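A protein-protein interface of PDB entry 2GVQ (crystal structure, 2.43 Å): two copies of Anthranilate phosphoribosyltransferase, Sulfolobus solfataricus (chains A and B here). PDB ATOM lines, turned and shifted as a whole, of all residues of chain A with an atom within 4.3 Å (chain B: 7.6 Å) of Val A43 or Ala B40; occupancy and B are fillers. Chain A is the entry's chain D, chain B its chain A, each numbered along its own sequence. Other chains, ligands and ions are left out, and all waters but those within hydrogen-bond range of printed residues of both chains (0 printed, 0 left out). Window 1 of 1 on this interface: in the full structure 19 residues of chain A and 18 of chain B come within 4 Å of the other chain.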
ATOM      1  N   SER A  39      27.537   2.471  21.251  1.00  0.00           N
ATOM      2  CA  SER A  39      26.794   3.655  21.647  1.00  0.00           C
ATOM      3  C   SER A  39      27.294   4.195  22.982  1.00  0.00           C
ATOM      4  O   SER A  39      27.687   5.361  23.089  1.00  0.00           O
ATOM      5  CB  SER A  39      25.308   3.307  21.739  1.00  0.00           C
ATOM      6  OG  SER A  39      24.543   4.420  22.134  1.00  0.00           O
ATOM      7  N   ALA A  40      27.279   3.334  24.000  1.00  0.00           N
ATOM      8  CA  ALA A  40      27.725   3.710  25.341  1.00  0.00           C
ATOM      9  C   ALA A  40      29.143   4.255  25.311  1.00  0.00           C
ATOM     10  O   ALA A  40      29.421   5.281  25.924  1.00  0.00           O
ATOM     11  CB  ALA A  40      27.643   2.505  26.284  1.00  0.00           C
ATOM     12  N   ILE A  41      30.038   3.578  24.594  1.00  0.00           N
ATOM     13  CA  ILE A  41      31.423   4.035  24.498  1.00  0.00           C
ATOM     14  C   ILE A  41      31.558   5.407  23.833  1.00  0.00           C
ATOM     15  O   ILE A  41      32.277   6.267  24.343  1.00  0.00           O
ATOM     16  CB  ILE A  41      32.316   3.020  23.734  1.00  0.00           C
ATOM     17  CG1 ILE A  41      32.479   1.750  24.576  1.00  0.00           C
ATOM     18  CG2 ILE A  41      33.685   3.630  23.458  1.00  0.00           C
ATOM     19  CD1 ILE A  41      33.247   0.638  23.879  1.00  0.00           C
ATOM     20  N   LEU A  42      30.871   5.620  22.713  1.00  0.00           N
ATOM     21  CA  LEU A  42      30.955   6.912  22.029  1.00  0.00           C
ATOM     22  C   LEU A  42      30.430   8.051  22.916  1.00  0.00           C
ATOM     23  O   LEU A  42      30.996   9.144  22.938  1.00  0.00           O
ATOM     24  CB  LEU A  42      30.203   6.861  20.688  1.00  0.00           C
ATOM     25  CG  LEU A  42      30.755   5.879  19.629  1.00  0.00           C
ATOM     26  CD1 LEU A  42      29.911   5.958  18.362  1.00  0.00           C
ATOM     27  CD2 LEU A  42      32.217   6.193  19.298  1.00  0.00           C
ATOM     28  N   VAL A  43      29.368   7.785  23.672  1.00  0.00           N
ATOM     29  CA  VAL A  43      28.792   8.787  24.571  1.00  0.00           C
ATOM     30  C   VAL A  43      29.701   9.038  25.784  1.00  0.00           C
ATOM     31  O   VAL A  43      29.917  10.183  26.198  1.00  0.00           O
ATOM     32  CB  VAL A  43      27.405   8.329  25.053  1.00  0.00           C
ATOM     33  CG1 VAL A  43      26.955   9.159  26.236  1.00  0.00           C
ATOM     34  CG2 VAL A  43      26.410   8.440  23.915  1.00  0.00           C
ATOM     35  N   ALA A  44      30.223   7.952  26.347  1.00  0.00           N
ATOM     36  CA  ALA A  44      31.118   8.021  27.493  1.00  0.00           C
ATOM     37  C   ALA A  44      32.365   8.790  27.093  1.00  0.00           C
ATOM     38  O   ALA A  44      32.853   9.646  27.837  1.00  0.00           O
ATOM     39  CB  ALA A  44      31.501   6.618  27.930  1.00  0.00           C
ATOM     40  N   LEU A  45      32.874   8.466  25.905  1.00  0.00           N
ATOM     41  CA  LEU A  45      34.076   9.090  25.352  1.00  0.00           C
ATOM     42  C   LEU A  45      33.869  10.598  25.243  1.00  0.00           C
ATOM     43  O   LEU A  45      34.721  11.394  25.652  1.00  0.00           O
ATOM     44  CB  LEU A  45      34.349   8.488  23.977  1.00  0.00           C
ATOM     45  CG  LEU A  45      35.750   8.104  23.489  1.00  0.00           C
ATOM     46  CD1 LEU A  45      36.671   7.702  24.623  1.00  0.00           C
ATOM     47  CD2 LEU A  45      35.583   6.946  22.508  1.00  0.00           C
ATOM     48  N   ARG A  46      32.723  11.000  24.706  1.00  0.00           N
ATOM     49  CA  ARG A  46      32.467  12.418  24.575  1.00  0.00           C
ATOM     50  C   ARG A  46      32.235  13.115  25.912  1.00  0.00           C
ATOM     51  O   ARG A  46      32.712  14.228  26.123  1.00  0.00           O
ATOM     52  CB  ARG A  46      31.270  12.682  23.671  1.00  0.00           C
ATOM     53  CG  ARG A  46      30.996  14.162  23.588  1.00  0.00           C
ATOM     54  CD  ARG A  46      29.996  14.506  22.532  1.00  0.00           C
ATOM     55  NE  ARG A  46      29.492  15.853  22.750  1.00  0.00           N
ATOM     56  CZ  ARG A  46      28.611  16.456  21.967  1.00  0.00           C
ATOM     57  NH1 ARG A  46      28.139  15.830  20.898  1.00  0.00           N
ATOM     58  NH2 ARG A  46      28.182  17.666  22.281  1.00  0.00           N
ATOM     59  N   MET A  47      31.492  12.472  26.809  1.00  0.00           N
ATOM     60  CA  MET A  47      31.215  13.071  28.112  1.00  0.00           C
ATOM     61  C   MET A  47      32.420  13.072  29.035  1.00  0.00           C
ATOM     62  O   MET A  47      32.492  13.860  29.971  1.00  0.00           O
ATOM     63  CB  MET A  47      30.022  12.383  28.766  1.00  0.00           C
ATOM     64  CG  MET A  47      28.749  12.632  27.987  1.00  0.00           C
ATOM     65  SD  MET A  47      27.283  12.398  28.940  1.00  0.00           S
ATOM     66  CE  MET A  47      27.498  13.652  30.223  1.00  0.00           C
ATOM     67  N   LEU A 167      22.217   7.973  17.119  1.00  0.00           N
ATOM     68  CA  LEU A 167      22.570   8.898  18.198  1.00  0.00           C
ATOM     69  C   LEU A 167      22.258  10.332  17.796  1.00  0.00           C
ATOM     70  O   LEU A 167      21.622  11.068  18.554  1.00  0.00           O
ATOM     71  CB  LEU A 167      24.057   8.796  18.562  1.00  0.00           C
ATOM     72  CG  LEU A 167      24.535   7.593  19.384  1.00  0.00           C
ATOM     73  CD1 LEU A 167      26.038   7.666  19.614  1.00  0.00           C
ATOM     74  CD2 LEU A 167      23.797   7.578  20.713  1.00  0.00           C
ATOM     75  N   LEU B   7      18.947  14.048  24.880  1.00  0.00           N
ATOM     76  CA  LEU B   7      20.296  13.517  24.810  1.00  0.00           C
ATOM     77  C   LEU B   7      21.334  14.639  24.790  1.00  0.00           C
ATOM     78  O   LEU B   7      22.267  14.651  25.596  1.00  0.00           O
ATOM     79  CB  LEU B   7      20.432  12.637  23.567  1.00  0.00           C
ATOM     80  CG  LEU B   7      21.769  11.931  23.326  1.00  0.00           C
ATOM     81  CD1 LEU B   7      22.191  11.129  24.560  1.00  0.00           C
ATOM     82  CD2 LEU B   7      21.629  11.021  22.119  1.00  0.00           C
ATOM     83  N   LEU B  10      21.657  16.215  28.098  1.00  0.00           N
ATOM     84  CA  LEU B  10      22.397  15.385  29.051  1.00  0.00           C
ATOM     85  C   LEU B  10      23.881  15.421  28.678  1.00  0.00           C
ATOM     86  O   LEU B  10      24.746  15.500  29.555  1.00  0.00           O
ATOM     87  CB  LEU B  10      21.898  13.937  29.013  1.00  0.00           C
ATOM     88  CG  LEU B  10      20.440  13.670  29.381  1.00  0.00           C
ATOM     89  CD1 LEU B  10      20.065  12.241  29.009  1.00  0.00           C
ATOM     90  CD2 LEU B  10      20.235  13.924  30.860  1.00  0.00           C
ATOM     91  N   ILE B  11      24.173  15.366  27.377  1.00  0.00           N
ATOM     92  CA  ILE B  11      25.559  15.412  26.912  1.00  0.00           C
ATOM     93  C   ILE B  11      26.227  16.692  27.401  1.00  0.00           C
ATOM     94  O   ILE B  11      27.416  16.697  27.688  1.00  0.00           O
ATOM     95  CB  ILE B  11      25.672  15.373  25.365  1.00  0.00           C
ATOM     96  CG1 ILE B  11      25.247  14.006  24.829  1.00  0.00           C
ATOM     97  CG2 ILE B  11      27.108  15.665  24.950  1.00  0.00           C
ATOM     98  CD1 ILE B  11      26.128  12.861  25.294  1.00  0.00           C
ATOM     99  N   PRO B  34      14.859   3.471  20.350  1.00  0.00           N
ATOM    100  CA  PRO B  34      15.840   2.492  19.871  1.00  0.00           C
ATOM    101  C   PRO B  34      16.841   2.143  20.963  1.00  0.00           C
ATOM    102  O   PRO B  34      17.234   3.005  21.752  1.00  0.00           O
ATOM    103  CB  PRO B  34      16.501   3.218  18.701  1.00  0.00           C
ATOM    104  CG  PRO B  34      15.428   4.192  18.245  1.00  0.00           C
ATOM    105  CD  PRO B  34      14.892   4.699  19.538  1.00  0.00           C
ATOM    106  N   GLU B  35      17.264   0.884  21.014  1.00  0.00           N
ATOM    107  CA  GLU B  35      18.221   0.456  22.033  1.00  0.00           C
ATOM    108  C   GLU B  35      19.452   1.340  22.055  1.00  0.00           C
ATOM    109  O   GLU B  35      19.981   1.662  23.121  1.00  0.00           O
ATOM    110  CB  GLU B  35      18.641  -0.997  21.815  1.00  0.00           C
ATOM    111  CG  GLU B  35      17.517  -1.990  22.082  1.00  0.00           C
ATOM    112  CD  GLU B  35      18.017  -3.416  22.290  1.00  0.00           C
ATOM    113  OE1 GLU B  35      18.746  -3.934  21.414  1.00  0.00           O
ATOM    114  OE2 GLU B  35      17.672  -4.015  23.337  1.00  0.00           O
ATOM    115  N   ILE B  36      19.900   1.746  20.876  1.00  0.00           N
ATOM    116  CA  ILE B  36      21.068   2.595  20.777  1.00  0.00           C
ATOM    117  C   ILE B  36      20.931   3.879  21.583  1.00  0.00           C
ATOM    118  O   ILE B  36      21.891   4.315  22.216  1.00  0.00           O
ATOM    119  CB  ILE B  36      21.366   2.938  19.315  1.00  0.00           C
ATOM    120  CG1 ILE B  36      21.874   1.694  18.597  1.00  0.00           C
ATOM    121  CG2 ILE B  36      22.390   4.051  19.239  1.00  0.00           C
ATOM    122  CD1 ILE B  36      21.991   1.848  17.103  1.00  0.00           C
ATOM    123  N   LEU B  37      19.747   4.480  21.567  1.00  0.00           N
ATOM    124  CA  LEU B  37      19.524   5.725  22.301  1.00  0.00           C
ATOM    125  C   LEU B  37      19.249   5.488  23.783  1.00  0.00           C
ATOM    126  O   LEU B  37      19.649   6.298  24.624  1.00  0.00           O
ATOM    127  CB  LEU B  37      18.381   6.519  21.655  1.00  0.00           C
ATOM    128  CG  LEU B  37      18.748   7.154  20.300  1.00  0.00           C
ATOM    129  CD1 LEU B  37      17.493   7.422  19.491  1.00  0.00           C
ATOM    130  CD2 LEU B  37      19.532   8.443  20.520  1.00  0.00           C
ATOM    131  N   VAL B  38      18.568   4.390  24.111  1.00  0.00           N
ATOM    132  CA  VAL B  38      18.309   4.088  25.522  1.00  0.00           C
ATOM    133  C   VAL B  38      19.691   3.954  26.163  1.00  0.00           C
ATOM    134  O   VAL B  38      19.965   4.515  27.236  1.00  0.00           O
ATOM    135  CB  VAL B  38      17.552   2.747  25.724  1.00  0.00           C
ATOM    136  CG1 VAL B  38      17.505   2.410  27.214  1.00  0.00           C
ATOM    137  CG2 VAL B  38      16.132   2.834  25.160  1.00  0.00           C
ATOM    138  N   SER B  39      20.562   3.220  25.479  1.00  0.00           N
ATOM    139  CA  SER B  39      21.920   3.011  25.948  1.00  0.00           C
ATOM    140  C   SER B  39      22.673   4.333  26.137  1.00  0.00           C
ATOM    141  O   SER B  39      23.260   4.584  27.203  1.00  0.00           O
ATOM    142  CB  SER B  39      22.676   2.118  24.968  1.00  0.00           C
ATOM    143  OG  SER B  39      24.034   1.988  25.356  1.00  0.00           O
ATOM    144  N   ALA B  40      22.657   5.178  25.107  1.00  0.00           N
ATOM    145  CA  ALA B  40      23.337   6.470  25.186  1.00  0.00           C
ATOM    146  C   ALA B  40      22.768   7.269  26.345  1.00  0.00           C
ATOM    147  O   ALA B  40      23.511   7.883  27.118  1.00  0.00           O
ATOM    148  CB  ALA B  40      23.156   7.245  23.891  1.00  0.00           C
ATOM    149  N   ILE B  41      21.441   7.254  26.457  1.00  0.00           N
ATOM    150  CA  ILE B  41      20.750   7.975  27.516  1.00  0.00           C
ATOM    151  C   ILE B  41      21.122   7.519  28.926  1.00  0.00           C
ATOM    152  O   ILE B  41      21.383   8.354  29.797  1.00  0.00           O
ATOM    153  CB  ILE B  41      19.218   7.873  27.352  1.00  0.00           C
ATOM    154  CG1 ILE B  41      18.799   8.599  26.067  1.00  0.00           C
ATOM    155  CG2 ILE B  41      18.522   8.474  28.574  1.00  0.00           C
ATOM    156  CD1 ILE B  41      17.322   8.558  25.772  1.00  0.00           C
ATOM    157  N   LEU B  42      21.136   6.208  29.165  1.00  0.00           N
ATOM    158  CA  LEU B  42      21.501   5.727  30.500  1.00  0.00           C
ATOM    159  C   LEU B  42      22.952   6.083  30.815  1.00  0.00           C
ATOM    160  O   LEU B  42      23.272   6.485  31.940  1.00  0.00           O
ATOM    161  CB  LEU B  42      21.283   4.213  30.623  1.00  0.00           C
ATOM    162  CG  LEU B  42      19.824   3.767  30.485  1.00  0.00           C
ATOM    163  CD1 LEU B  42      19.742   2.267  30.488  1.00  0.00           C
ATOM    164  CD2 LEU B  42      18.994   4.353  31.604  1.00  0.00           C
ATOM    165  N   VAL B  43      23.827   5.964  29.822  1.00  0.00           N
ATOM    166  CA  VAL B  43      25.233   6.289  30.031  1.00  0.00           C
ATOM    167  C   VAL B  43      25.457   7.781  30.295  1.00  0.00           C
ATOM    168  O   VAL B  43      26.294   8.157  31.127  1.00  0.00           O
ATOM    169  CB  VAL B  43      26.095   5.842  28.833  1.00  0.00           C
ATOM    170  CG1 VAL B  43      27.509   6.384  28.973  1.00  0.00           C
ATOM    171  CG2 VAL B  43      26.125   4.309  28.754  1.00  0.00           C
ATOM    172  N   ALA B  44      24.709   8.636  29.603  1.00  0.00           N
ATOM    173  CA  ALA B  44      24.861  10.077  29.800  1.00  0.00           C
ATOM    174  C   ALA B  44      24.410  10.437  31.218  1.00  0.00           C
ATOM    175  O   ALA B  44      25.054  11.233  31.908  1.00  0.00           O
ATOM    176  CB  ALA B  44      24.035  10.840  28.764  1.00  0.00           C
ATOM    177  N   LEU B  45      23.297   9.828  31.627  1.00  0.00           N
ATOM    178  CA  LEU B  45      22.701  10.027  32.947  1.00  0.00           C
ATOM    179  C   LEU B  45      23.703   9.637  34.031  1.00  0.00           C
ATOM    180  O   LEU B  45      23.936  10.392  34.981  1.00  0.00           O
ATOM    181  CB  LEU B  45      21.430   9.173  33.065  1.00  0.00           C
ATOM    182  CG  LEU B  45      20.041   9.804  33.239  1.00  0.00           C
ATOM    183  CD1 LEU B  45      19.925  11.093  32.467  1.00  0.00           C
ATOM    184  CD2 LEU B  45      18.987   8.807  32.777  1.00  0.00           C
ATOM    185  N   ARG B  46      24.306   8.460  33.890  1.00  0.00           N
ATOM    186  CA  ARG B  46      25.276   8.042  34.878  1.00  0.00           C
ATOM    187  C   ARG B  46      26.480   8.972  34.900  1.00  0.00           C
ATOM    188  O   ARG B  46      26.885   9.440  35.960  1.00  0.00           O
ATOM    189  CB  ARG B  46      25.754   6.609  34.635  1.00  0.00           C
ATOM    190  CG  ARG B  46      26.872   6.268  35.597  1.00  0.00           C
ATOM    191  CD  ARG B  46      27.133   4.800  35.728  1.00  0.00           C
ATOM    192  NE  ARG B  46      28.173   4.560  36.722  1.00  0.00           N
ATOM    193  CZ  ARG B  46      28.512   3.360  37.173  1.00  0.00           C
ATOM    194  NH1 ARG B  46      27.887   2.282  36.722  1.00  0.00           N
ATOM    195  NH2 ARG B  46      29.492   3.237  38.061  1.00  0.00           N
ATOM    196  N   MET B  47      27.057   9.244  33.733  1.00  0.00           N
ATOM    197  CA  MET B  47      28.223  10.120  33.670  1.00  0.00           C
ATOM    198  C   MET B  47      27.946  11.567  34.039  1.00  0.00           C
ATOM    199  O   MET B  47      28.832  12.264  34.516  1.00  0.00           O
ATOM    200  CB  MET B  47      28.866  10.041  32.293  1.00  0.00           C
ATOM    201  CG  MET B  47      29.347   8.639  31.996  1.00  0.00           C
ATOM    202  SD  MET B  47      30.754   8.625  30.953  1.00  0.00           S
ATOM    203  CE  MET B  47      31.861   9.708  31.847  1.00  0.00           C
ATOM    204  N   VAL B 163      19.352  -3.891  27.172  1.00  0.00           N
ATOM    205  CA  VAL B 163      20.281  -2.778  27.283  1.00  0.00           C
ATOM    206  C   VAL B 163      21.066  -2.838  28.573  1.00  0.00           C
ATOM    207  O   VAL B 163      22.293  -2.683  28.572  1.00  0.00           O
ATOM    208  CB  VAL B 163      19.549  -1.421  27.188  1.00  0.00           C
ATOM    209  CG1 VAL B 163      20.452  -0.294  27.664  1.00  0.00           C
ATOM    210  CG2 VAL B 163      19.132  -1.170  25.743  1.00  0.00           C
ATOM    211  N   LEU B 167      25.186  -3.469  28.748  1.00  0.00           N
ATOM    212  CA  LEU B 167      26.024  -2.446  29.361  1.00  0.00           C
ATOM    213  C   LEU B 167      26.776  -3.032  30.544  1.00  0.00           C
ATOM    214  O   LEU B 167      27.942  -2.713  30.764  1.00  0.00           O
ATOM    215  CB  LEU B 167      25.172  -1.268  29.836  1.00  0.00           C
ATOM    216  CG  LEU B 167      24.511  -0.463  28.726  1.00  0.00           C
ATOM    217  CD1 LEU B 167      23.632   0.616  29.315  1.00  0.00           C
ATOM    218  CD2 LEU B 167      25.604   0.127  27.853  1.00  0.00           C
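Ala A40 touches Val B43, and with the chains exchanged Val A43 touches Ala B40.
Ala A40 touches Leu B167, and with the chains exchanged Leu A167 touches Ala B40.
Val B43 touches its own counterpart, Val A43.
Ala A44 touches Met B47, and with the chains exchanged Met A47 touches Ala B44.
10 positions are printed for both chains.
Ala A40 touches Ser B39.
Val B43 touches Ala A40 (CG2 to CB, 3.4 Å).
Ala A40 touches Leu B167.
Ile B11 touches Val A43.
NE of Arg A46 touches CG2 of Ile B11, at 3.2 Å.
Leu B10 touches Met A47 (O to CE, 3.4 Å).
Met A47 touches Ile B11.
Leu B7 touches Leu A167.
Leu B37 touches Leu A167.
Ala B40 touches Leu A167.
Printed residues of chain B that touch a printed residue of chain A: Leu B7, Leu B10, Ile B11, Ile B36, Leu B37, Ser B39, Ala B40, Val B43, Ala B44, Met B47 and Leu B167.
Val A43 touches three residues of chain B.
Of the printed residues of chain A, Leu B10 touches Met A47.
Of the printed residues of chain A, Leu B37 touches Leu A167 (3.9 Å).
Ala B40 touches three residues of chain A.
Ile B41 touches none of the printed residues of chain A.
Of the printed residues of chain A, Met B47 touches Ala A44.
The nearest residue of chain B that does not touch Val A43 is Ala B44 (4.1 Å).
The nearest printed residue of chain A that does not touch Ala B40 is Ala A40 (5.1 Å).
The backbone carbonyl oxygen (O) of Ile B36 lies within hydrogen-bond range of the side-chain hydroxyl (OG) of Ser A39 (2.7 Å).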
